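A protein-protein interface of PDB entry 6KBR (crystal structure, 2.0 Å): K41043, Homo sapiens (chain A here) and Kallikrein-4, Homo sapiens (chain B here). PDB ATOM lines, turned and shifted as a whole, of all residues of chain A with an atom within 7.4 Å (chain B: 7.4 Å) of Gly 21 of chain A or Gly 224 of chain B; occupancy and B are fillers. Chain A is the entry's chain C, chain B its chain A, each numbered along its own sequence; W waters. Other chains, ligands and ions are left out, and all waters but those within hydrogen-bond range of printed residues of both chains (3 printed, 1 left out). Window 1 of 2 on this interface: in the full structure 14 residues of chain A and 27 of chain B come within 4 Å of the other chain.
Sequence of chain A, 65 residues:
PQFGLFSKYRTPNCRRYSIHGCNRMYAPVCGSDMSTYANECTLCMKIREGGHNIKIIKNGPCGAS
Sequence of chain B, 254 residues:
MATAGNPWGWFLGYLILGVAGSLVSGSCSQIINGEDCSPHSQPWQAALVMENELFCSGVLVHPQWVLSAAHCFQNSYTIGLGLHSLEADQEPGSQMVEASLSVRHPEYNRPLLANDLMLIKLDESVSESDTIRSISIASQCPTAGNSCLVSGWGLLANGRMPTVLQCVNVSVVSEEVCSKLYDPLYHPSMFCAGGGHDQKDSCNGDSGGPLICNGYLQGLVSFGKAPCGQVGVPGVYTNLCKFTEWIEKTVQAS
The guanidinium group (NH1) of Arg 24 of chain A is in salt-bridge range of the side-chain carboxylate (OD1) of Asp 201 of chain B (2.8 Å). The side-chain amide oxygen (OD1) of Asn 204 of chain B lies close to the backbone carbonyl oxygen (O) of Asn 23 of chain A. OG of Ser 202 of chain B lies within hydrogen-bond range of NH1 of Arg 24 of chain A. NZ of Lys 225 of chain B is in hydrogen-bond range of O of His 20 of chain A, 3.0 Å away. O of Ser 222 of chain B sits at hydrogen-bond distance from N of Arg 24 of chain A, 3.1 Å away. O of Gly 224 of chain B lies within hydrogen-bond range of N of Cys 22 of chain A (2.8 Å). The backbone NH of Ala 226 of chain B sits close to the side-chain sulfur of Met 45 of chain A, at 3.5 Å. The guanidinium group (NE) of Arg 24 of chain A sits close to the backbone NH (N) of Gly 224 of chain B, 3.5 Å away.
The backbone carbonyl oxygen (O) of Val 236 of chain B sits at hydrogen-bond distance from the backbone NH (N) of Ser 222 of chain B, 3.1 Å away. The side-chain sulfur (SG) of Cys 22 of chain A lies within hydrogen-bond range of the backbone NH (N) of Thr 42 of chain A, 3.7 Å away. The side-chain hydroxyl (OG) of Ser 18 of chain A lies within hydrogen-bond range of the backbone NH (N) of His 20 of chain A, 2.9 Å away. OG of Ser 202 of chain B sits at hydrogen-bond distance from OH of Tyr 237 of chain B (3.2 Å). The backbone carbonyl oxygen of Phe 223 of chain B is in hydrogen-bond range of the backbone NH of Val 236 of chain B, at 2.9 Å. The backbone carbonyl oxygen (O) of Ala 226 of chain B sits close to the side-chain amide oxygen (OE1) of Gln 230 of chain B.
Of the 11 printed residues of chain A, 8 touch a printed residue of chain B. Of the 21 printed residues of chain B, 14 touch a printed residue of chain A. Among the printed residues, 25 pairs touch across the chains. Among the printed residues, Asp or Glu carboxylates within 4 Å of a Lys or Arg side-chain nitrogen of the other chain: Arg 24 of chain A with Asp 201 of chain B (2.8 Å).
Among the printed residues, pairs that only touch across the chains: Cys 22 of chain A with Phe 223 of chain B (3.2 Å), Gly 21 of chain A with Gly 224 of chain B (3.3 Å), His 20 of chain A with Tyr 182 of chain B (3.3 Å), Arg 24 of chain A with Asn 204 of chain B (3.3 Å), Asn 23 of chain A with Ser 222 of chain B (3.4 Å), His 20 of chain A with Leu 185 of chain B (3.5 Å), Ser 18 of chain A with Leu 185 of chain B (3.5 Å), Asn 23 of chain A with Phe 223 of chain B (3.6 Å), Arg 24 of chain A with Phe 223 of chain B (3.7 Å), Gly 21 of chain A with Leu 185 of chain B (3.8 Å), Ser 18 of chain A with Leu 112 of chain B (3.8 Å), Arg 24 of chain A with Gly 235 of chain B (3.8 Å), Arg 24 of chain A with Val 221 of chain B (3.9 Å), Gly 21 of chain A with Leu 113 of chain B (3.9 Å), Gly 21 of chain A with Phe 223 of chain B (3.9 Å), Thr 42 of chain A with Ala 226 of chain B (3.9 Å) and Thr 42 of chain A with Asn 204 of chain B (3.9 Å).
Water W1 lies within hydrogen-bond range of the guanidinium group of Arg 24 of chain A, the backbone carbonyl oxygen of Lys 225 of chain B and the side-chain sulfur of Cys 228 of chain B. Water W3 lies within hydrogen-bond range of the backbone carbonyl oxygen (O) of Val 236 of chain B (2.8 Å), the side-chain hydroxyl (OG) of Ser 202 of chain B (3.1 Å) and the guanidinium group (NH1) of Arg 24 of chain A (3.1 Å). Water W2 lies within hydrogen-bond range of O of Pro 227 of chain B (2.9 Å), O of Lys 225 of chain B (3.0 Å) and NH2 of Arg 24 of chain A (3.5 Å).
Ile 19 of chain A touches none of the printed residues of chain B. Of chain B, only Leu 113, Leu 185, Phe 223 and Gly 224 come within 4 Å of Gly 21 of chain A. Of the printed residues of chain B, Met 45 of chain A touches Ala 226. Printed residues of chain A within 4 Å of Asn 204 of chain B: Asn 23, Arg 24 and Thr 42. Printed residues of chain A within 4 Å of Gly 224 of chain B: Gly 21, Cys 22 and Arg 24. Printed residues of chain A within 4 Å of Lys 225 of chain B: His 20. Of the printed residues of chain A, Ala 226 of chain B touches Thr 42 (3.9 Å) and Met 45 (3.3 Å). Val 236 of chain B touches none of the printed residues of chain A. The nearest residue of chain B that does not touch Gly 21 of chain A is Tyr 182 of chain B (4.9 Å). The nearest printed residue of chain A that does not touch Leu 113 of chain B is Ser 18 of chain A (4.4 Å).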
ATOM      1  N   TYR A  17      -2.747  14.977 -10.341  1.00  0.00           N
ATOM      2  CA  TYR A  17      -1.707  14.118 -10.938  1.00  0.00           C
ATOM      3  C   TYR A  17      -2.245  13.370 -12.113  1.00  0.00           C
ATOM      4  O   TYR A  17      -3.450  13.161 -12.211  1.00  0.00           O
ATOM      5  CB  TYR A  17      -1.156  13.084  -9.925  1.00  0.00           C
ATOM      6  CG  TYR A  17      -0.620  13.769  -8.724  1.00  0.00           C
ATOM      7  CD1 TYR A  17       0.587  14.482  -8.761  1.00  0.00           C
ATOM      8  CD2 TYR A  17      -1.351  13.787  -7.540  1.00  0.00           C
ATOM      9  CE1 TYR A  17       1.042  15.170  -7.624  1.00  0.00           C
ATOM     10  CE2 TYR A  17      -0.895  14.458  -6.428  1.00  0.00           C
ATOM     11  CZ  TYR A  17       0.294  15.146  -6.481  1.00  0.00           C
ATOM     12  OH  TYR A  17       0.680  15.816  -5.323  1.00  0.00           O
ATOM     13  N   SER A  18      -1.338  12.912 -12.969  1.00  0.00           N
ATOM     14  CA  SER A  18      -1.695  11.920 -13.971  1.00  0.00           C
ATOM     15  C   SER A  18      -1.754  10.474 -13.434  1.00  0.00           C
ATOM     16  O   SER A  18      -0.935  10.043 -12.621  1.00  0.00           O
ATOM     17  CB  SER A  18      -0.768  12.036 -15.183  1.00  0.00           C
ATOM     18  OG  SER A  18      -0.886  10.944 -16.083  1.00  0.00           O
ATOM     19  N   ILE A  19      -2.718   9.694 -13.924  1.00  0.00           N
ATOM     20  CA  ILE A  19      -2.745   8.248 -13.627  1.00  0.00           C
ATOM     21  C   ILE A  19      -1.644   7.499 -14.382  1.00  0.00           C
ATOM     22  O   ILE A  19      -1.339   6.332 -14.065  1.00  0.00           O
ATOM     23  CB  ILE A  19      -4.131   7.597 -13.949  1.00  0.00           C
ATOM     24  CG1 ILE A  19      -4.392   7.542 -15.467  1.00  0.00           C
ATOM     25  CG2 ILE A  19      -5.249   8.388 -13.223  1.00  0.00           C
ATOM     26  CD1 ILE A  19      -5.789   7.104 -15.869  1.00  0.00           C
ATOM     27  N   HIS A  20      -1.057   8.130 -15.395  1.00  0.00           N
ATOM     28  CA  HIS A  20      -0.070   7.465 -16.287  1.00  0.00           C
ATOM     29  C   HIS A  20       1.418   7.611 -15.904  1.00  0.00           C
ATOM     30  O   HIS A  20       2.274   6.986 -16.534  1.00  0.00           O
ATOM     31  CB  HIS A  20      -0.227   8.013 -17.716  1.00  0.00           C
ATOM     32  CG  HIS A  20      -1.600   7.820 -18.253  1.00  0.00           C
ATOM     33  ND1 HIS A  20      -2.460   8.870 -18.501  1.00  0.00           N
ATOM     34  CD2 HIS A  20      -2.292   6.693 -18.498  1.00  0.00           C
ATOM     35  CE1 HIS A  20      -3.621   8.397 -18.902  1.00  0.00           C
ATOM     36  NE2 HIS A  20      -3.543   7.078 -18.921  1.00  0.00           N
ATOM     37  N   GLY A  21       1.724   8.514 -14.971  1.00  0.00           N
ATOM     38  CA  GLY A  21       3.073   8.624 -14.500  1.00  0.00           C
ATOM     39  C   GLY A  21       3.166   9.526 -13.294  1.00  0.00           C
ATOM     40  O   GLY A  21       2.337  10.429 -13.120  1.00  0.00           O
ATOM     41  N   CYS A  22       4.205   9.294 -12.502  1.00  0.00           N
ATOM     42  CA  CYS A  22       4.554  10.119 -11.364  1.00  0.00           C
ATOM     43  C   CYS A  22       6.036  10.498 -11.463  1.00  0.00           C
ATOM     44  O   CYS A  22       6.859   9.617 -11.730  1.00  0.00           O
ATOM     45  CB  CYS A  22       4.370   9.310 -10.073  1.00  0.00           C
ATOM     46  SG  CYS A  22       2.660   9.119  -9.612  1.00  0.00           S
ATOM     47  N   ASN A  23       6.362  11.784 -11.199  1.00  0.00           N
ATOM     48  CA  ASN A  23       7.753  12.235 -11.181  1.00  0.00           C
ATOM     49  C   ASN A  23       8.494  11.501 -10.101  1.00  0.00           C
ATOM     50  O   ASN A  23       7.862  10.969  -9.211  1.00  0.00           O
ATOM     51  CB  ASN A  23       7.948  13.762 -11.150  1.00  0.00           C
ATOM     52  CG  ASN A  23       7.554  14.496  -9.820  1.00  0.00           C
ATOM     53  OD1 ASN A  23       7.082  15.681  -9.920  1.00  0.00           O
ATOM     54  ND2 ASN A  23       7.798  13.925  -8.631  1.00  0.00           N
ATOM     55  N   ARG A  24       9.809  11.421 -10.230  1.00  0.00           N
ATOM     56  CA  ARG A  24      10.617  10.583  -9.378  1.00  0.00           C
ATOM     57  C   ARG A  24      11.394  11.383  -8.312  1.00  0.00           C
ATOM     58  O   ARG A  24      12.516  11.011  -7.930  1.00  0.00           O
ATOM     59  CB  ARG A  24      11.510   9.712 -10.267  1.00  0.00           C
ATOM     60  CG  ARG A  24      10.707   8.491 -10.701  1.00  0.00           C
ATOM     61  CD  ARG A  24      11.321   7.705 -11.833  1.00  0.00           C
ATOM     62  NE  ARG A  24      10.571   6.430 -12.005  1.00  0.00           N
ATOM     63  CZ  ARG A  24      10.992   5.396 -12.740  1.00  0.00           C
ATOM     64  NH1 ARG A  24      12.199   5.383 -13.335  1.00  0.00           N
ATOM     65  NH2 ARG A  24      10.198   4.354 -12.850  1.00  0.00           N
ATOM     66  N   CYS A  41       1.936  11.660  -5.430  1.00  0.00           N
ATOM     67  CA  CYS A  41       1.490  11.095  -6.672  1.00  0.00           C
ATOM     68  C   CYS A  41       1.490   9.561  -6.579  1.00  0.00           C
ATOM     69  O   CYS A  41       0.533   8.910  -7.053  1.00  0.00           O
ATOM     70  CB  CYS A  41       2.316  11.614  -7.843  1.00  0.00           C
ATOM     71  SG  CYS A  41       1.821  10.977  -9.473  1.00  0.00           S
ATOM     72  N   THR A  42       2.494   9.015  -5.890  1.00  0.00           N
ATOM     73  CA  THR A  42       2.649   7.552  -5.725  1.00  0.00           C
ATOM     74  C   THR A  42       1.554   6.956  -4.834  1.00  0.00           C
ATOM     75  O   THR A  42       1.032   5.844  -5.102  1.00  0.00           O
ATOM     76  CB  THR A  42       4.045   7.220  -5.221  1.00  0.00           C
ATOM     77  OG1 THR A  42       4.991   7.725  -6.174  1.00  0.00           O
ATOM     78  CG2 THR A  42       4.273   5.766  -5.115  1.00  0.00           C
ATOM     79  N   MET A  45      -1.482   6.753  -7.049  1.00  0.00           N
ATOM     80  CA  MET A  45      -1.416   5.537  -7.813  1.00  0.00           C
ATOM     81  C   MET A  45      -1.881   4.264  -6.980  1.00  0.00           C
ATOM     82  O   MET A  45      -2.676   3.466  -7.428  1.00  0.00           O
ATOM     83  CB  MET A  45      -0.005   5.399  -8.405  1.00  0.00           C
ATOM     84  CG  MET A  45       0.153   6.208  -9.715  1.00  0.00           C
ATOM     85  SD  MET A  45       1.617   5.782 -10.700  1.00  0.00           S
ATOM     86  CE  MET A  45       1.060   4.210 -11.367  1.00  0.00           C
ATOM     87  N   LEU B 112       1.468  18.031 -19.751  1.00  0.00           N
ATOM     88  CA  LEU B 112       1.769  17.535 -18.428  1.00  0.00           C
ATOM     89  C   LEU B 112       3.040  16.631 -18.492  1.00  0.00           C
ATOM     90  O   LEU B 112       3.168  15.817 -19.412  1.00  0.00           O
ATOM     91  CB  LEU B 112       0.524  16.785 -17.938  1.00  0.00           C
ATOM     92  CG  LEU B 112       0.388  16.232 -16.540  1.00  0.00           C
ATOM     93  CD1 LEU B 112       0.602  17.278 -15.423  1.00  0.00           C
ATOM     94  CD2 LEU B 112      -1.015  15.618 -16.473  1.00  0.00           C
ATOM     95  N   LEU B 113       3.980  16.873 -17.585  1.00  0.00           N
ATOM     96  CA  LEU B 113       5.251  16.076 -17.410  1.00  0.00           C
ATOM     97  C   LEU B 113       6.364  16.323 -18.466  1.00  0.00           C
ATOM     98  O   LEU B 113       7.502  15.776 -18.349  1.00  0.00           O
ATOM     99  CB  LEU B 113       4.907  14.561 -17.261  1.00  0.00           C
ATOM    100  CG  LEU B 113       4.065  14.245 -16.005  1.00  0.00           C
ATOM    101  CD1 LEU B 113       3.452  12.858 -15.938  1.00  0.00           C
ATOM    102  CD2 LEU B 113       4.912  14.426 -14.776  1.00  0.00           C
ATOM    103  N   TYR B 182       3.010   5.097 -22.516  1.00  0.00           N
ATOM    104  CA  TYR B 182       2.665   6.346 -21.800  1.00  0.00           C
ATOM    105  C   TYR B 182       1.619   7.274 -22.412  1.00  0.00           C
ATOM    106  O   TYR B 182       1.424   8.412 -21.945  1.00  0.00           O
ATOM    107  CB  TYR B 182       3.932   7.133 -21.471  1.00  0.00           C
ATOM    108  CG  TYR B 182       4.697   6.428 -20.395  1.00  0.00           C
ATOM    109  CD1 TYR B 182       4.350   6.604 -19.064  1.00  0.00           C
ATOM    110  CD2 TYR B 182       5.725   5.583 -20.704  1.00  0.00           C
ATOM    111  CE1 TYR B 182       5.039   5.989 -18.070  1.00  0.00           C
ATOM    112  CE2 TYR B 182       6.436   4.940 -19.723  1.00  0.00           C
ATOM    113  CZ  TYR B 182       6.109   5.147 -18.409  1.00  0.00           C
ATOM    114  OH  TYR B 182       6.804   4.518 -17.403  1.00  0.00           O
ATOM    115  N   LEU B 185       0.461  10.861 -22.557  1.00  0.00           N
ATOM    116  CA  LEU B 185       1.431  11.677 -21.881  1.00  0.00           C
ATOM    117  C   LEU B 185       2.781  11.757 -22.671  1.00  0.00           C
ATOM    118  O   LEU B 185       3.603  12.645 -22.412  1.00  0.00           O
ATOM    119  CB  LEU B 185       1.665  11.030 -20.517  1.00  0.00           C
ATOM    120  CG  LEU B 185       1.934  11.654 -19.170  1.00  0.00           C
ATOM    121  CD1 LEU B 185       0.750  12.547 -18.772  1.00  0.00           C
ATOM    122  CD2 LEU B 185       2.213  10.504 -18.163  1.00  0.00           C
ATOM    123  N   ASP B 201      15.744  -0.311 -13.163  1.00  0.00           N
ATOM    124  CA  ASP B 201      15.052   1.004 -13.331  1.00  0.00           C
ATOM    125  C   ASP B 201      15.716   2.020 -12.431  1.00  0.00           C
ATOM    126  O   ASP B 201      16.500   1.653 -11.537  1.00  0.00           O
ATOM    127  CB  ASP B 201      13.578   0.830 -12.911  1.00  0.00           C
ATOM    128  CG  ASP B 201      12.618   1.883 -13.464  1.00  0.00           C
ATOM    129  OD1 ASP B 201      13.015   2.851 -14.145  1.00  0.00           O
ATOM    130  OD2 ASP B 201      11.408   1.717 -13.191  1.00  0.00           O
ATOM    131  N   SER B 202      15.416   3.302 -12.662  1.00  0.00           N
ATOM    132  CA  SER B 202      15.544   4.294 -11.633  1.00  0.00           C
ATOM    133  C   SER B 202      14.211   4.311 -10.821  1.00  0.00           C
ATOM    134  O   SER B 202      13.287   3.537 -11.091  1.00  0.00           O
ATOM    135  CB  SER B 202      15.882   5.641 -12.276  1.00  0.00           C
ATOM    136  OG  SER B 202      14.880   5.925 -13.215  1.00  0.00           O
ATOM    137  N   ASN B 204      12.055   6.664  -7.289  1.00  0.00           N
ATOM    138  CA  ASN B 204      11.867   7.894  -6.566  1.00  0.00           C
ATOM    139  C   ASN B 204      13.102   8.263  -5.789  1.00  0.00           C
ATOM    140  O   ASN B 204      13.744   7.378  -5.219  1.00  0.00           O
ATOM    141  CB  ASN B 204      10.641   7.787  -5.679  1.00  0.00           C
ATOM    142  CG  ASN B 204       9.392   7.578  -6.530  1.00  0.00           C
ATOM    143  OD1 ASN B 204       9.104   8.396  -7.381  1.00  0.00           O
ATOM    144  ND2 ASN B 204       8.731   6.478  -6.377  1.00  0.00           N
ATOM    145  N   VAL B 221      16.730  11.504 -15.135  1.00  0.00           N
ATOM    146  CA  VAL B 221      15.607  10.742 -14.624  1.00  0.00           C
ATOM    147  C   VAL B 221      14.433  11.720 -14.457  1.00  0.00           C
ATOM    148  O   VAL B 221      14.598  12.711 -13.769  1.00  0.00           O
ATOM    149  CB  VAL B 221      15.897  10.129 -13.239  1.00  0.00           C
ATOM    150  CG1 VAL B 221      14.644   9.477 -12.688  1.00  0.00           C
ATOM    151  CG2 VAL B 221      17.108   9.175 -13.269  1.00  0.00           C
ATOM    152  N   SER B 222      13.253  11.388 -14.962  1.00  0.00           N
ATOM    153  CA  SER B 222      12.107  12.252 -14.911  1.00  0.00           C
ATOM    154  C   SER B 222      10.904  11.638 -14.199  1.00  0.00           C
ATOM    155  O   SER B 222      10.504  12.121 -13.175  1.00  0.00           O
ATOM    156  CB  SER B 222      11.748  12.728 -16.350  1.00  0.00           C
ATOM    157  OG  SER B 222      10.633  13.629 -16.341  1.00  0.00           O
ATOM    158  N   PHE B 223      10.310  10.581 -14.767  1.00  0.00           N
ATOM    159  CA  PHE B 223       9.089   9.999 -14.158  1.00  0.00           C
ATOM    160  C   PHE B 223       8.940   8.545 -14.501  1.00  0.00           C
ATOM    161  O   PHE B 223       9.643   8.052 -15.340  1.00  0.00           O
ATOM    162  CB  PHE B 223       7.807  10.843 -14.520  1.00  0.00           C
ATOM    163  CG  PHE B 223       7.332  10.730 -15.936  1.00  0.00           C
ATOM    164  CD1 PHE B 223       7.791  11.631 -16.911  1.00  0.00           C
ATOM    165  CD2 PHE B 223       6.307   9.815 -16.291  1.00  0.00           C
ATOM    166  CE1 PHE B 223       7.299  11.570 -18.179  1.00  0.00           C
ATOM    167  CE2 PHE B 223       5.798   9.782 -17.578  1.00  0.00           C
ATOM    168  CZ  PHE B 223       6.311  10.623 -18.522  1.00  0.00           C
ATOM    169  N   GLY B 224       7.998   7.873 -13.859  1.00  0.00           N
ATOM    170  CA  GLY B 224       7.646   6.493 -14.212  1.00  0.00           C
ATOM    171  C   GLY B 224       6.348   6.075 -13.554  1.00  0.00           C
ATOM    172  O   GLY B 224       5.543   6.925 -13.216  1.00  0.00           O
ATOM    173  N   LYS B 225       6.134   4.781 -13.388  1.00  0.00           N
ATOM    174  CA  LYS B 225       4.888   4.281 -12.775  1.00  0.00           C
ATOM    175  C   LYS B 225       5.223   3.690 -11.393  1.00  0.00           C
ATOM    176  O   LYS B 225       6.393   3.574 -10.995  1.00  0.00           O
ATOM    177  CB  LYS B 225       4.210   3.261 -13.672  1.00  0.00           C
ATOM    178  CG  LYS B 225       3.660   3.776 -14.997  1.00  0.00           C
ATOM    179  CD  LYS B 225       2.846   2.755 -15.792  1.00  0.00           C
ATOM    180  CE  LYS B 225       2.825   3.027 -17.304  1.00  0.00           C
ATOM    181  NZ  LYS B 225       2.014   4.243 -17.653  1.00  0.00           N
ATOM    182  N   ALA B 226       4.183   3.371 -10.642  1.00  0.00           N
ATOM    183  CA  ALA B 226       4.310   2.792  -9.317  1.00  0.00           C
ATOM    184  C   ALA B 226       3.822   1.300  -9.294  1.00  0.00           C
ATOM    185  O   ALA B 226       2.735   1.031  -9.732  1.00  0.00           O
ATOM    186  CB  ALA B 226       3.518   3.652  -8.351  1.00  0.00           C
ATOM    187  N   PRO B 227       4.629   0.319  -8.867  1.00  0.00           N
ATOM    188  CA  PRO B 227       6.004   0.513  -8.431  1.00  0.00           C
ATOM    189  C   PRO B 227       6.986   0.735  -9.556  1.00  0.00           C
ATOM    190  O   PRO B 227       6.666   0.552 -10.740  1.00  0.00           O
ATOM    191  CB  PRO B 227       6.331  -0.818  -7.746  1.00  0.00           C
ATOM    192  CG  PRO B 227       5.506  -1.821  -8.520  1.00  0.00           C
ATOM    193  CD  PRO B 227       4.235  -1.113  -8.836  1.00  0.00           C
ATOM    194  N   CYS B 228       8.191   1.130  -9.167  1.00  0.00           N
ATOM    195  CA  CYS B 228       9.320   1.163 -10.069  1.00  0.00           C
ATOM    196  C   CYS B 228       9.733  -0.261 -10.451  1.00  0.00           C
ATOM    197  O   CYS B 228       9.370  -1.181  -9.783  1.00  0.00           O
ATOM    198  CB  CYS B 228      10.531   1.836  -9.404  1.00  0.00           C
ATOM    199  SG  CYS B 228      10.207   3.494  -8.731  1.00  0.00           S
ATOM    200  N   GLN B 230       8.838  -2.370 -12.774  1.00  0.00           N
ATOM    201  CA  GLN B 230       7.828  -3.272 -13.322  1.00  0.00           C
ATOM    202  C   GLN B 230       8.325  -3.936 -14.606  1.00  0.00           C
ATOM    203  O   GLN B 230       8.819  -3.247 -15.509  1.00  0.00           O
ATOM    204  CB  GLN B 230       6.493  -2.561 -13.598  1.00  0.00           C
ATOM    205  CG  GLN B 230       5.785  -2.005 -12.373  1.00  0.00           C
ATOM    206  CD  GLN B 230       4.510  -1.280 -12.749  1.00  0.00           C
ATOM    207  OE1 GLN B 230       4.296  -0.109 -12.434  1.00  0.00           O
ATOM    208  NE2 GLN B 230       3.642  -1.978 -13.352  1.00  0.00           N
ATOM    209  N   VAL B 233       7.816  -2.326 -18.221  1.00  0.00           N
ATOM    210  CA  VAL B 233       7.458  -0.898 -18.145  1.00  0.00           C
ATOM    211  C   VAL B 233       8.764  -0.096 -18.016  1.00  0.00           C
ATOM    212  O   VAL B 233       9.391  -0.163 -16.968  1.00  0.00           O
ATOM    213  CB  VAL B 233       6.526  -0.609 -16.925  1.00  0.00           C
ATOM    214  CG1 VAL B 233       6.215   0.872 -16.834  1.00  0.00           C
ATOM    215  CG2 VAL B 233       5.278  -1.456 -16.923  1.00  0.00           C
ATOM    216  N   PRO B 234       9.210   0.625 -19.080  1.00  0.00           N
ATOM    217  CA  PRO B 234      10.421   1.436 -18.918  1.00  0.00           C
ATOM    218  C   PRO B 234      10.178   2.706 -18.116  1.00  0.00           C
ATOM    219  O   PRO B 234       9.034   3.202 -18.050  1.00  0.00           O
ATOM    220  CB  PRO B 234      10.797   1.806 -20.366  1.00  0.00           C
ATOM    221  CG  PRO B 234       9.507   1.828 -21.070  1.00  0.00           C
ATOM    222  CD  PRO B 234       8.627   0.789 -20.427  1.00  0.00           C
ATOM    223  N   GLY B 235      11.270   3.246 -17.553  1.00  0.00           N
ATOM    224  CA  GLY B 235      11.260   4.574 -16.969  1.00  0.00           C
ATOM    225  C   GLY B 235      11.335   5.653 -18.026  1.00  0.00           C
ATOM    226  O   GLY B 235      11.698   5.373 -19.184  1.00  0.00           O
ATOM    227  N   VAL B 236      10.976   6.887 -17.649  1.00  0.00           N
ATOM    228  CA  VAL B 236      10.975   7.994 -18.578  1.00  0.00           C
ATOM    229  C   VAL B 236      12.009   9.019 -18.205  1.00  0.00           C
ATOM    230  O   VAL B 236      12.137   9.367 -17.039  1.00  0.00           O
ATOM    231  CB  VAL B 236       9.585   8.629 -18.843  1.00  0.00           C
ATOM    232  CG1 VAL B 236       9.655   9.498 -20.090  1.00  0.00           C
ATOM    233  CG2 VAL B 236       8.564   7.537 -19.107  1.00  0.00           C
ATOM    234  N   TYR B 237      12.707   9.500 -19.226  1.00  0.00           N
ATOM    235  CA  TYR B 237      13.893  10.362 -19.092  1.00  0.00           C
ATOM    236  C   TYR B 237      13.733  11.633 -19.928  1.00  0.00           C
ATOM    237  O   TYR B 237      13.109  11.614 -20.964  1.00  0.00           O
ATOM    238  CB  TYR B 237      15.177   9.606 -19.497  1.00  0.00           C
ATOM    239  CG  TYR B 237      15.434   8.445 -18.630  1.00  0.00           C
ATOM    240  CD1 TYR B 237      14.771   7.256 -18.823  1.00  0.00           C
ATOM    241  CD2 TYR B 237      16.335   8.544 -17.536  1.00  0.00           C
ATOM    242  CE1 TYR B 237      15.006   6.149 -17.974  1.00  0.00           C
ATOM    243  CE2 TYR B 237      16.542   7.477 -16.658  1.00  0.00           C
ATOM    244  CZ  TYR B 237      15.896   6.272 -16.882  1.00  0.00           C
ATOM    245  OH  TYR B 237      16.133   5.212 -16.034  1.00  0.00           O
HETATM  246  O   HOH W   1       8.187   5.806 -10.885  1.00  0.00           O
HETATM  247  O   HOH W   2       7.752   1.910 -13.114  1.00  0.00           O
HETATM  248  O   HOH W   3      13.245   7.658 -15.153  1.00  0.00           O
